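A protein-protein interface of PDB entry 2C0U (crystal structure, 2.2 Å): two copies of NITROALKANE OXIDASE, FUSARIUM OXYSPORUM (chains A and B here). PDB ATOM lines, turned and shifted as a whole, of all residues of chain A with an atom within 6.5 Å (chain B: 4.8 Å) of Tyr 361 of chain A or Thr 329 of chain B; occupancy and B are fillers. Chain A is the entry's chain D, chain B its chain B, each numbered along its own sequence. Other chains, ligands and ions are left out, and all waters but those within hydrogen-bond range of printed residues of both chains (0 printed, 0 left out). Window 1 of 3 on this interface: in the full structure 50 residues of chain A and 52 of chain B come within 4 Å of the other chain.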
ATOM      1  N   ILE A 325      16.006  -6.705  15.402  1.00  0.00           N
ATOM      2  CA  ILE A 325      16.685  -7.934  15.732  1.00  0.00           C
ATOM      3  C   ILE A 325      16.717  -8.898  14.546  1.00  0.00           C
ATOM      4  O   ILE A 325      17.755  -9.502  14.259  1.00  0.00           O
ATOM      5  CB  ILE A 325      16.015  -8.587  16.956  1.00  0.00           C
ATOM      6  CG1 ILE A 325      16.259  -7.708  18.184  1.00  0.00           C
ATOM      7  CG2 ILE A 325      16.568  -9.976  17.204  1.00  0.00           C
ATOM      8  CD1 ILE A 325      15.613  -8.241  19.451  1.00  0.00           C
ATOM      9  N   ARG A 326      15.601  -9.026  13.833  1.00  0.00           N
ATOM     10  CA  ARG A 326      15.562  -9.939  12.694  1.00  0.00           C
ATOM     11  C   ARG A 326      16.570  -9.533  11.640  1.00  0.00           C
ATOM     12  O   ARG A 326      17.308 -10.370  11.125  1.00  0.00           O
ATOM     13  CB  ARG A 326      14.160  -9.986  12.077  1.00  0.00           C
ATOM     14  CG  ARG A 326      13.132 -10.693  12.939  1.00  0.00           C
ATOM     15  CD  ARG A 326      11.744 -10.551  12.332  1.00  0.00           C
ATOM     16  NE  ARG A 326      10.709 -11.045  13.234  1.00  0.00           N
ATOM     17  CZ  ARG A 326       9.663 -10.330  13.639  1.00  0.00           C
ATOM     18  NH1 ARG A 326       9.501  -9.073  13.233  1.00  0.00           N
ATOM     19  NH2 ARG A 326       8.778 -10.875  14.461  1.00  0.00           N
ATOM     20  N   LEU A 327      16.600  -8.246  11.322  1.00  0.00           N
ATOM     21  CA  LEU A 327      17.528  -7.729  10.326  1.00  0.00           C
ATOM     22  C   LEU A 327      18.979  -7.896  10.783  1.00  0.00           C
ATOM     23  O   LEU A 327      19.844  -8.269   9.993  1.00  0.00           O
ATOM     24  CB  LEU A 327      17.244  -6.246  10.073  1.00  0.00           C
ATOM     25  CG  LEU A 327      15.940  -5.905   9.353  1.00  0.00           C
ATOM     26  CD1 LEU A 327      15.637  -4.414   9.515  1.00  0.00           C
ATOM     27  CD2 LEU A 327      16.053  -6.297   7.876  1.00  0.00           C
ATOM     28  N   THR A 329      20.299 -10.069  13.132  1.00  0.00           N
ATOM     29  CA  THR A 329      20.677 -11.463  13.123  1.00  0.00           C
ATOM     30  C   THR A 329      20.830 -11.974  11.694  1.00  0.00           C
ATOM     31  O   THR A 329      21.720 -12.779  11.421  1.00  0.00           O
ATOM     32  CB  THR A 329      19.641 -12.317  13.846  1.00  0.00           C
ATOM     33  OG1 THR A 329      18.326 -12.020  13.348  1.00  0.00           O
ATOM     34  CG2 THR A 329      19.708 -12.046  15.332  1.00  0.00           C
ATOM     35  N   SER A 330      19.986 -11.496  10.776  1.00  0.00           N
ATOM     36  CA  SER A 330      20.060 -11.943   9.389  1.00  0.00           C
ATOM     37  C   SER A 330      21.341 -11.518   8.696  1.00  0.00           C
ATOM     38  O   SER A 330      21.944 -12.309   7.968  1.00  0.00           O
ATOM     39  CB  SER A 330      18.868 -11.425   8.562  1.00  0.00           C
ATOM     40  OG  SER A 330      17.633 -11.961   9.009  1.00  0.00           O
ATOM     41  N   LEU A 332      24.232 -10.811  10.062  1.00  0.00           N
ATOM     42  CA  LEU A 332      25.350 -11.542  10.629  1.00  0.00           C
ATOM     43  C   LEU A 332      25.415 -12.950  10.053  1.00  0.00           C
ATOM     44  O   LEU A 332      26.494 -13.457   9.750  1.00  0.00           O
ATOM     45  CB  LEU A 332      25.228 -11.622  12.146  1.00  0.00           C
ATOM     46  CG  LEU A 332      25.296 -10.266  12.862  1.00  0.00           C
ATOM     47  CD1 LEU A 332      25.224 -10.477  14.351  1.00  0.00           C
ATOM     48  CD2 LEU A 332      26.582  -9.563  12.504  1.00  0.00           C
ATOM     49  N   LEU A 333      24.250 -13.568   9.892  1.00  0.00           N
ATOM     50  CA  LEU A 333      24.162 -14.916   9.363  1.00  0.00           C
ATOM     51  C   LEU A 333      24.647 -14.930   7.928  1.00  0.00           C
ATOM     52  O   LEU A 333      25.416 -15.804   7.533  1.00  0.00           O
ATOM     53  CB  LEU A 333      22.714 -15.416   9.407  1.00  0.00           C
ATOM     54  CG  LEU A 333      22.463 -16.839   9.905  1.00  0.00           C
ATOM     55  CD1 LEU A 333      21.057 -17.278   9.478  1.00  0.00           C
ATOM     56  CD2 LEU A 333      23.516 -17.785   9.350  1.00  0.00           C
ATOM     57  N   MET A 356      22.201 -23.131   3.728  1.00  0.00           N
ATOM     58  CA  MET A 356      20.780 -23.464   3.848  1.00  0.00           C
ATOM     59  C   MET A 356      20.174 -22.711   5.036  1.00  0.00           C
ATOM     60  O   MET A 356      19.078 -22.153   4.941  1.00  0.00           O
ATOM     61  CB  MET A 356      20.572 -24.972   4.066  1.00  0.00           C
ATOM     62  CG  MET A 356      21.190 -25.869   2.999  1.00  0.00           C
ATOM     63  SD  MET A 356      20.456 -25.561   1.241  1.00  0.00           S
ATOM     64  CE  MET A 356      21.758 -24.324   0.518  1.00  0.00           C
ATOM     65  N   GLN A 357      20.892 -22.713   6.159  1.00  0.00           N
ATOM     66  CA  GLN A 357      20.455 -22.032   7.374  1.00  0.00           C
ATOM     67  C   GLN A 357      20.141 -20.570   7.101  1.00  0.00           C
ATOM     68  O   GLN A 357      19.126 -20.051   7.552  1.00  0.00           O
ATOM     69  CB  GLN A 357      21.546 -22.090   8.449  1.00  0.00           C
ATOM     70  CG  GLN A 357      21.600 -23.382   9.234  1.00  0.00           C
ATOM     71  CD  GLN A 357      22.725 -23.379  10.256  1.00  0.00           C
ATOM     72  OE1 GLN A 357      23.861 -23.743   9.950  1.00  0.00           O
ATOM     73  NE2 GLN A 357      22.415 -22.952  11.474  1.00  0.00           N
ATOM     74  N   THR A 358      21.032 -19.915   6.368  1.00  0.00           N
ATOM     75  CA  THR A 358      20.888 -18.507   6.040  1.00  0.00           C
ATOM     76  C   THR A 358      19.651 -18.244   5.190  1.00  0.00           C
ATOM     77  O   THR A 358      18.856 -17.340   5.473  1.00  0.00           O
ATOM     78  CB  THR A 358      22.121 -18.003   5.273  1.00  0.00           C
ATOM     79  OG1 THR A 358      23.301 -18.331   6.016  1.00  0.00           O
ATOM     80  CG2 THR A 358      22.041 -16.496   5.069  1.00  0.00           C
ATOM     81  N   LYS A 359      19.494 -19.040   4.142  1.00  0.00           N
ATOM     82  CA  LYS A 359      18.368 -18.883   3.241  1.00  0.00           C
ATOM     83  C   LYS A 359      17.045 -19.096   3.985  1.00  0.00           C
ATOM     84  O   LYS A 359      16.107 -18.316   3.826  1.00  0.00           O
ATOM     85  CB  LYS A 359      18.511 -19.873   2.081  1.00  0.00           C
ATOM     86  CG  LYS A 359      17.788 -19.471   0.801  1.00  0.00           C
ATOM     87  CD  LYS A 359      16.294 -19.695   0.893  1.00  0.00           C
ATOM     88  CE  LYS A 359      15.616 -19.388  -0.435  1.00  0.00           C
ATOM     89  NZ  LYS A 359      14.170 -19.736  -0.372  1.00  0.00           N
ATOM     90  N   ILE A 360      16.986 -20.134   4.814  1.00  0.00           N
ATOM     91  CA  ILE A 360      15.774 -20.460   5.565  1.00  0.00           C
ATOM     92  C   ILE A 360      15.400 -19.375   6.577  1.00  0.00           C
ATOM     93  O   ILE A 360      14.248 -18.926   6.642  1.00  0.00           O
ATOM     94  CB  ILE A 360      15.949 -21.805   6.312  1.00  0.00           C
ATOM     95  CG1 ILE A 360      16.160 -22.941   5.293  1.00  0.00           C
ATOM     96  CG2 ILE A 360      14.744 -22.070   7.212  1.00  0.00           C
ATOM     97  CD1 ILE A 360      16.607 -24.277   5.917  1.00  0.00           C
ATOM     98  N   TYR A 361      16.379 -18.950   7.363  1.00  0.00           N
ATOM     99  CA  TYR A 361      16.141 -17.944   8.381  1.00  0.00           C
ATOM    100  C   TYR A 361      15.851 -16.560   7.828  1.00  0.00           C
ATOM    101  O   TYR A 361      14.851 -15.951   8.171  1.00  0.00           O
ATOM    102  CB  TYR A 361      17.349 -17.839   9.310  1.00  0.00           C
ATOM    103  CG  TYR A 361      17.169 -16.834  10.430  1.00  0.00           C
ATOM    104  CD1 TYR A 361      16.299 -17.091  11.490  1.00  0.00           C
ATOM    105  CD2 TYR A 361      17.852 -15.620  10.420  1.00  0.00           C
ATOM    106  CE1 TYR A 361      16.117 -16.163  12.517  1.00  0.00           C
ATOM    107  CE2 TYR A 361      17.681 -14.685  11.438  1.00  0.00           C
ATOM    108  CZ  TYR A 361      16.808 -14.960  12.478  1.00  0.00           C
ATOM    109  OH  TYR A 361      16.602 -14.018  13.455  1.00  0.00           O
ATOM    110  N   THR A 362      16.745 -16.065   6.983  1.00  0.00           N
ATOM    111  CA  THR A 362      16.588 -14.732   6.449  1.00  0.00           C
ATOM    112  C   THR A 362      15.290 -14.510   5.689  1.00  0.00           C
ATOM    113  O   THR A 362      14.593 -13.519   5.933  1.00  0.00           O
ATOM    114  CB  THR A 362      17.794 -14.337   5.577  1.00  0.00           C
ATOM    115  OG1 THR A 362      17.840 -15.143   4.393  1.00  0.00           O
ATOM    116  CG2 THR A 362      19.085 -14.528   6.370  1.00  0.00           C
ATOM    117  N   THR A 363      14.948 -15.424   4.788  1.00  0.00           N
ATOM    118  CA  THR A 363      13.731 -15.276   4.008  1.00  0.00           C
ATOM    119  C   THR A 363      12.477 -15.371   4.881  1.00  0.00           C
ATOM    120  O   THR A 363      11.518 -14.616   4.690  1.00  0.00           O
ATOM    121  CB  THR A 363      13.675 -16.321   2.844  1.00  0.00           C
ATOM    122  OG1 THR A 363      13.591 -17.658   3.363  1.00  0.00           O
ATOM    123  CG2 THR A 363      14.928 -16.209   1.999  1.00  0.00           C
ATOM    124  N   ASP A 364      12.487 -16.270   5.860  1.00  0.00           N
ATOM    125  CA  ASP A 364      11.331 -16.411   6.735  1.00  0.00           C
ATOM    126  C   ASP A 364      11.080 -15.186   7.622  1.00  0.00           C
ATOM    127  O   ASP A 364       9.933 -14.737   7.748  1.00  0.00           O
ATOM    128  CB  ASP A 364      11.467 -17.652   7.631  1.00  0.00           C
ATOM    129  CG  ASP A 364      11.076 -18.953   6.920  1.00  0.00           C
ATOM    130  OD1 ASP A 364      10.377 -18.891   5.885  1.00  0.00           O
ATOM    131  OD2 ASP A 364      11.454 -20.045   7.405  1.00  0.00           O
ATOM    132  N   VAL A 365      12.130 -14.653   8.248  1.00  0.00           N
ATOM    133  CA  VAL A 365      11.958 -13.502   9.128  1.00  0.00           C
ATOM    134  C   VAL A 365      11.777 -12.210   8.358  1.00  0.00           C
ATOM    135  O   VAL A 365      11.234 -11.250   8.885  1.00  0.00           O
ATOM    136  CB  VAL A 365      13.141 -13.331  10.113  1.00  0.00           C
ATOM    137  CG1 VAL A 365      13.255 -14.571  11.004  1.00  0.00           C
ATOM    138  CG2 VAL A 365      14.431 -13.027   9.341  1.00  0.00           C
ATOM    139  N   ALA A 366      12.237 -12.179   7.114  1.00  0.00           N
ATOM    140  CA  ALA A 366      12.080 -10.981   6.307  1.00  0.00           C
ATOM    141  C   ALA A 366      10.582 -10.699   6.092  1.00  0.00           C
ATOM    142  O   ALA A 366      10.151  -9.543   6.081  1.00  0.00           O
ATOM    143  CB  ALA A 366      12.786 -11.153   4.981  1.00  0.00           C
ATOM    144  N   GLU A 368       8.122 -11.653   8.174  1.00  0.00           N
ATOM    145  CA  GLU A 368       7.601 -11.195   9.463  1.00  0.00           C
ATOM    146  C   GLU A 368       7.976  -9.735   9.744  1.00  0.00           C
ATOM    147  O   GLU A 368       7.201  -8.992  10.353  1.00  0.00           O
ATOM    148  CB  GLU A 368       8.140 -12.072  10.593  1.00  0.00           C
ATOM    149  CG  GLU A 368       7.753 -13.539  10.497  1.00  0.00           C
ATOM    150  CD  GLU A 368       8.601 -14.423  11.400  1.00  0.00           C
ATOM    151  OE1 GLU A 368       8.713 -14.117  12.606  1.00  0.00           O
ATOM    152  OE2 GLU A 368       9.157 -15.430  10.906  1.00  0.00           O
ATOM    153  N   ASN A 405      12.039 -23.058   0.828  1.00  0.00           N
ATOM    154  CA  ASN A 405      12.511 -23.509   2.136  1.00  0.00           C
ATOM    155  C   ASN A 405      11.933 -24.854   2.561  1.00  0.00           C
ATOM    156  O   ASN A 405      12.640 -25.700   3.101  1.00  0.00           O
ATOM    157  CB  ASN A 405      12.141 -22.492   3.221  1.00  0.00           C
ATOM    158  CG  ASN A 405      12.764 -21.128   3.001  1.00  0.00           C
ATOM    159  OD1 ASN A 405      12.425 -20.171   3.699  1.00  0.00           O
ATOM    160  ND2 ASN A 405      13.678 -21.029   2.044  1.00  0.00           N
ATOM    161  N   ILE B 325      19.320 -23.119  13.891  1.00  0.00           N
ATOM    162  CA  ILE B 325      19.312 -21.732  13.415  1.00  0.00           C
ATOM    163  C   ILE B 325      19.302 -20.733  14.578  1.00  0.00           C
ATOM    164  O   ILE B 325      20.027 -19.742  14.573  1.00  0.00           O
ATOM    165  CB  ILE B 325      18.094 -21.482  12.513  1.00  0.00           C
ATOM    166  CG1 ILE B 325      18.284 -22.204  11.182  1.00  0.00           C
ATOM    167  CG2 ILE B 325      17.918 -20.001  12.252  1.00  0.00           C
ATOM    168  CD1 ILE B 325      17.057 -22.128  10.284  1.00  0.00           C
ATOM    169  N   ARG B 326      18.472 -20.995  15.574  1.00  0.00           N
ATOM    170  CA  ARG B 326      18.403 -20.116  16.725  1.00  0.00           C
ATOM    171  C   ARG B 326      19.776 -20.029  17.413  1.00  0.00           C
ATOM    172  O   ARG B 326      20.235 -18.942  17.780  1.00  0.00           O
ATOM    173  CB  ARG B 326      17.374 -20.649  17.713  1.00  0.00           C
ATOM    174  CG  ARG B 326      15.947 -20.633  17.185  1.00  0.00           C
ATOM    175  CD  ARG B 326      15.051 -21.501  18.063  1.00  0.00           C
ATOM    176  NE  ARG B 326      13.654 -21.426  17.655  1.00  0.00           N
ATOM    177  CZ  ARG B 326      12.801 -22.447  17.695  1.00  0.00           C
ATOM    178  NH1 ARG B 326      13.193 -23.646  18.123  1.00  0.00           N
ATOM    179  NH2 ARG B 326      11.545 -22.269  17.303  1.00  0.00           N
ATOM    180  N   LEU B 327      20.421 -21.183  17.584  1.00  0.00           N
ATOM    181  CA  LEU B 327      21.719 -21.249  18.235  1.00  0.00           C
ATOM    182  C   LEU B 327      22.767 -20.547  17.399  1.00  0.00           C
ATOM    183  O   LEU B 327      23.605 -19.813  17.917  1.00  0.00           O
ATOM    184  CB  LEU B 327      22.125 -22.710  18.475  1.00  0.00           C
ATOM    185  CG  LEU B 327      21.323 -23.462  19.547  1.00  0.00           C
ATOM    186  CD1 LEU B 327      21.574 -24.958  19.438  1.00  0.00           C
ATOM    187  CD2 LEU B 327      21.703 -22.955  20.934  1.00  0.00           C
ATOM    188  N   GLU B 328      22.700 -20.755  16.094  1.00  0.00           N
ATOM    189  CA  GLU B 328      23.657 -20.158  15.182  1.00  0.00           C
ATOM    190  C   GLU B 328      23.566 -18.635  15.182  1.00  0.00           C
ATOM    191  O   GLU B 328      24.586 -17.942  15.318  1.00  0.00           O
ATOM    192  CB  GLU B 328      23.410 -20.677  13.772  1.00  0.00           C
ATOM    193  CG  GLU B 328      24.637 -20.656  12.892  1.00  0.00           C
ATOM    194  CD  GLU B 328      25.599 -21.798  13.193  1.00  0.00           C
ATOM    195  OE1 GLU B 328      25.356 -22.947  12.745  1.00  0.00           O
ATOM    196  OE2 GLU B 328      26.605 -21.547  13.887  1.00  0.00           O
ATOM    197  N   THR B 329      22.345 -18.121  15.018  1.00  0.00           N
ATOM    198  CA  THR B 329      22.119 -16.673  14.999  1.00  0.00           C
ATOM    199  C   THR B 329      22.441 -16.045  16.356  1.00  0.00           C
ATOM    200  O   THR B 329      22.921 -14.925  16.417  1.00  0.00           O
ATOM    201  CB  THR B 329      20.644 -16.310  14.611  1.00  0.00           C
ATOM    202  OG1 THR B 329      19.734 -17.022  15.461  1.00  0.00           O
ATOM    203  CG2 THR B 329      20.363 -16.635  13.148  1.00  0.00           C
ATOM    204  N   SER B 330      22.174 -16.773  17.433  1.00  0.00           N
ATOM    205  CA  SER B 330      22.460 -16.287  18.766  1.00  0.00           C
ATOM    206  C   SER B 330      23.948 -16.056  19.015  1.00  0.00           C
ATOM    207  O   SER B 330      24.347 -15.006  19.531  1.00  0.00           O
ATOM    208  CB  SER B 330      21.959 -17.269  19.815  1.00  0.00           C
ATOM    209  OG  SER B 330      20.559 -17.233  19.912  1.00  0.00           O
ATOM    210  N   ARG B 331      24.770 -17.039  18.661  1.00  0.00           N
ATOM    211  CA  ARG B 331      26.203 -16.931  18.894  1.00  0.00           C
ATOM    212  C   ARG B 331      26.769 -15.761  18.120  1.00  0.00           C
ATOM    213  O   ARG B 331      27.552 -14.973  18.649  1.00  0.00           O
ATOM    214  CB  ARG B 331      26.926 -18.230  18.506  1.00  0.00           C
ATOM    215  CG  ARG B 331      28.406 -18.229  18.864  1.00  0.00           C
ATOM    216  CD  ARG B 331      29.067 -19.544  18.519  1.00  0.00           C
ATOM    217  NE  ARG B 331      28.420 -20.667  19.189  1.00  0.00           N
ATOM    218  CZ  ARG B 331      27.781 -21.636  18.544  1.00  0.00           C
ATOM    219  NH1 ARG B 331      27.703 -21.604  17.220  1.00  0.00           N
ATOM    220  NH2 ARG B 331      27.238 -22.636  19.218  1.00  0.00           N
ATOM    221  N   LEU B 332      26.360 -15.638  16.867  1.00  0.00           N
ATOM    222  CA  LEU B 332      26.820 -14.543  16.033  1.00  0.00           C
ATOM    223  C   LEU B 332      26.438 -13.188  16.636  1.00  0.00           C
ATOM    224  O   LEU B 332      27.212 -12.229  16.572  1.00  0.00           O
ATOM    225  CB  LEU B 332      26.213 -14.679  14.634  1.00  0.00           C
ATOM    226  CG  LEU B 332      27.003 -15.430  13.554  1.00  0.00           C
ATOM    227  CD1 LEU B 332      27.633 -16.669  14.127  1.00  0.00           C
ATOM    228  CD2 LEU B 332      26.076 -15.790  12.409  1.00  0.00           C
ATOM    229  N   LEU B 333      25.243 -13.114  17.222  1.00  0.00           N
ATOM    230  CA  LEU B 333      24.772 -11.868  17.817  1.00  0.00           C
ATOM    231  C   LEU B 333      25.609 -11.535  19.033  1.00  0.00           C
ATOM    232  O   LEU B 333      25.989 -10.386  19.221  1.00  0.00           O
ATOM    233  CB  LEU B 333      23.306 -11.963  18.246  1.00  0.00           C
ATOM    234  CG  LEU B 333      22.315 -10.902  17.748  1.00  0.00           C
ATOM    235  CD1 LEU B 333      21.102 -10.933  18.678  1.00  0.00           C
ATOM    236  CD2 LEU B 333      22.933  -9.499  17.719  1.00  0.00           C
ATOM    237  N   TYR B 361      16.936 -11.258  22.177  1.00  0.00           N
ATOM    238  CA  TYR B 361      16.874 -12.336  21.197  1.00  0.00           C
ATOM    239  C   TYR B 361      17.345 -13.699  21.731  1.00  0.00           C
ATOM    240  O   TYR B 361      16.592 -14.681  21.694  1.00  0.00           O
ATOM    241  CB  TYR B 361      17.716 -11.979  19.972  1.00  0.00           C
ATOM    242  CG  TYR B 361      17.667 -13.037  18.895  1.00  0.00           C
ATOM    243  CD1 TYR B 361      16.512 -13.228  18.137  1.00  0.00           C
ATOM    244  CD2 TYR B 361      18.755 -13.879  18.670  1.00  0.00           C
ATOM    245  CE1 TYR B 361      16.437 -14.229  17.182  1.00  0.00           C
ATOM    246  CE2 TYR B 361      18.694 -14.889  17.715  1.00  0.00           C
ATOM    247  CZ  TYR B 361      17.532 -15.057  16.974  1.00  0.00           C
ATOM    248  OH  TYR B 361      17.468 -16.029  16.010  1.00  0.00           O
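NE2 of Gln 357 of chain A is in hydrogen-bond range of OE1 of Glu 328 of chain B (3.2 Å). The side-chain hydroxyl (OH) of Tyr 361 of chain A sits at hydrogen-bond distance from the side-chain hydroxyl (OH) of Tyr 361 of chain B, 3.4 Å away.
O of Ile 325 of chain B lies within hydrogen-bond range of OG1 of Thr 329 of chain B (2.9 Å). The backbone carbonyl oxygen (O) of Arg 326 of chain B lies within hydrogen-bond range of the side-chain hydroxyl (OG1) of Thr 329 of chain B (3.1 Å). The side-chain hydroxyl of Thr 329 of chain B sits at hydrogen-bond distance from the side-chain hydroxyl of Tyr 361 of chain B (2.5 Å). OG1 of Thr 329 of chain A is in hydrogen-bond range of O of Ile 325 of chain A, 2.7 Å away. O of Arg 326 of chain A sits at hydrogen-bond distance from OG1 of Thr 329 of chain A (2.9 Å). OH of Tyr 361 of chain A lies within hydrogen-bond range of OG1 of Thr 329 of chain A, at 2.6 Å.
Tyr 361 of chain B touches Ile 325 of chain A (CD1 to CG2, 3.4 Å). Thr 329 of chain A touches Leu 333 of chain B. Tyr 361 of chain B touches Thr 329 of chain A. Leu 332 of chain A touches Leu 332 of chain B (CD1 to O, 3.5 Å). CA of Leu 333 of chain B touches CD1 of Leu 332 of chain A, at 3.8 Å. Leu 333 of chain A touches Thr 329 of chain B (CD1 to CG2, 3.8 Å). CD2 of Leu 332 of chain B touches CA of Leu 333 of chain A, 3.7 Å away. CA of Ile 325 of chain B touches NE2 of Gln 357 of chain A (3.9 Å). Ile 325 of chain B touches Ile 360 of chain A. Tyr 361 of chain A touches Thr 329 of chain B (CE2 to CG2, 3.7 Å).
Of the printed residues of chain B, Leu 333 of chain A touches Thr 329 and Leu 332. Met 356 of chain A touches none of the printed residues of chain B. Thr 358 of chain A touches none of the printed residues of chain B. Of the printed residues of chain B, Ile 360 of chain A touches Ile 325. Tyr 361 of chain A touches just these residues of chain B: Ile 325, Thr 329 and Tyr 361. Thr 329 of chain B touches just these residues of chain A: Leu 333 (3.8 Å) and Tyr 361 (3.7 Å). Printed residues of chain A within 4 Å of Leu 333 of chain B: Thr 329 and Leu 332. Printed residues of chain A within 4 Å of Tyr 361 of chain B: Ile 325 (3.4 Å), Thr 329 (3.8 Å) and Tyr 361 (3.4 Å). The nearest printed residue of chain A that does not touch Tyr 361 of chain B is Arg 326 of chain A (6.1 Å).
Of the 20 printed residues of chain A, 7 touch a printed residue of chain B. Hydrophobic or aromatic side chains of chain A that line the printed part of chain B: Ile 325, Leu 332, Leu 333, Ile 360 and Tyr 361. Among the printed residues, 13 pairs touch across the chains. Among the printed residues, no Asp or Glu carboxylate lies within 4 Å of a Lys or Arg side-chain nitrogen of the other chain.
Ile 325 of chain A touches Tyr 361 of chain B, and with the chains exchanged Tyr 361 of chain A touches Ile 325 of chain B. Thr 329 of chain A touches Leu 333 of chain B, and with the chains exchanged Leu 333 of chain A touches Thr 329 of chain B. Thr 329 of chain A touches Tyr 361 of chain B, and with the chains exchanged Tyr 361 of chain A touches Thr 329 of chain B. Leu 332 of chain B touches its own counterpart, Leu 332 of chain A. Of the 13 pairs that touch across the chains among the printed residues, 10 have their exchanged pair printed and touching as well.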
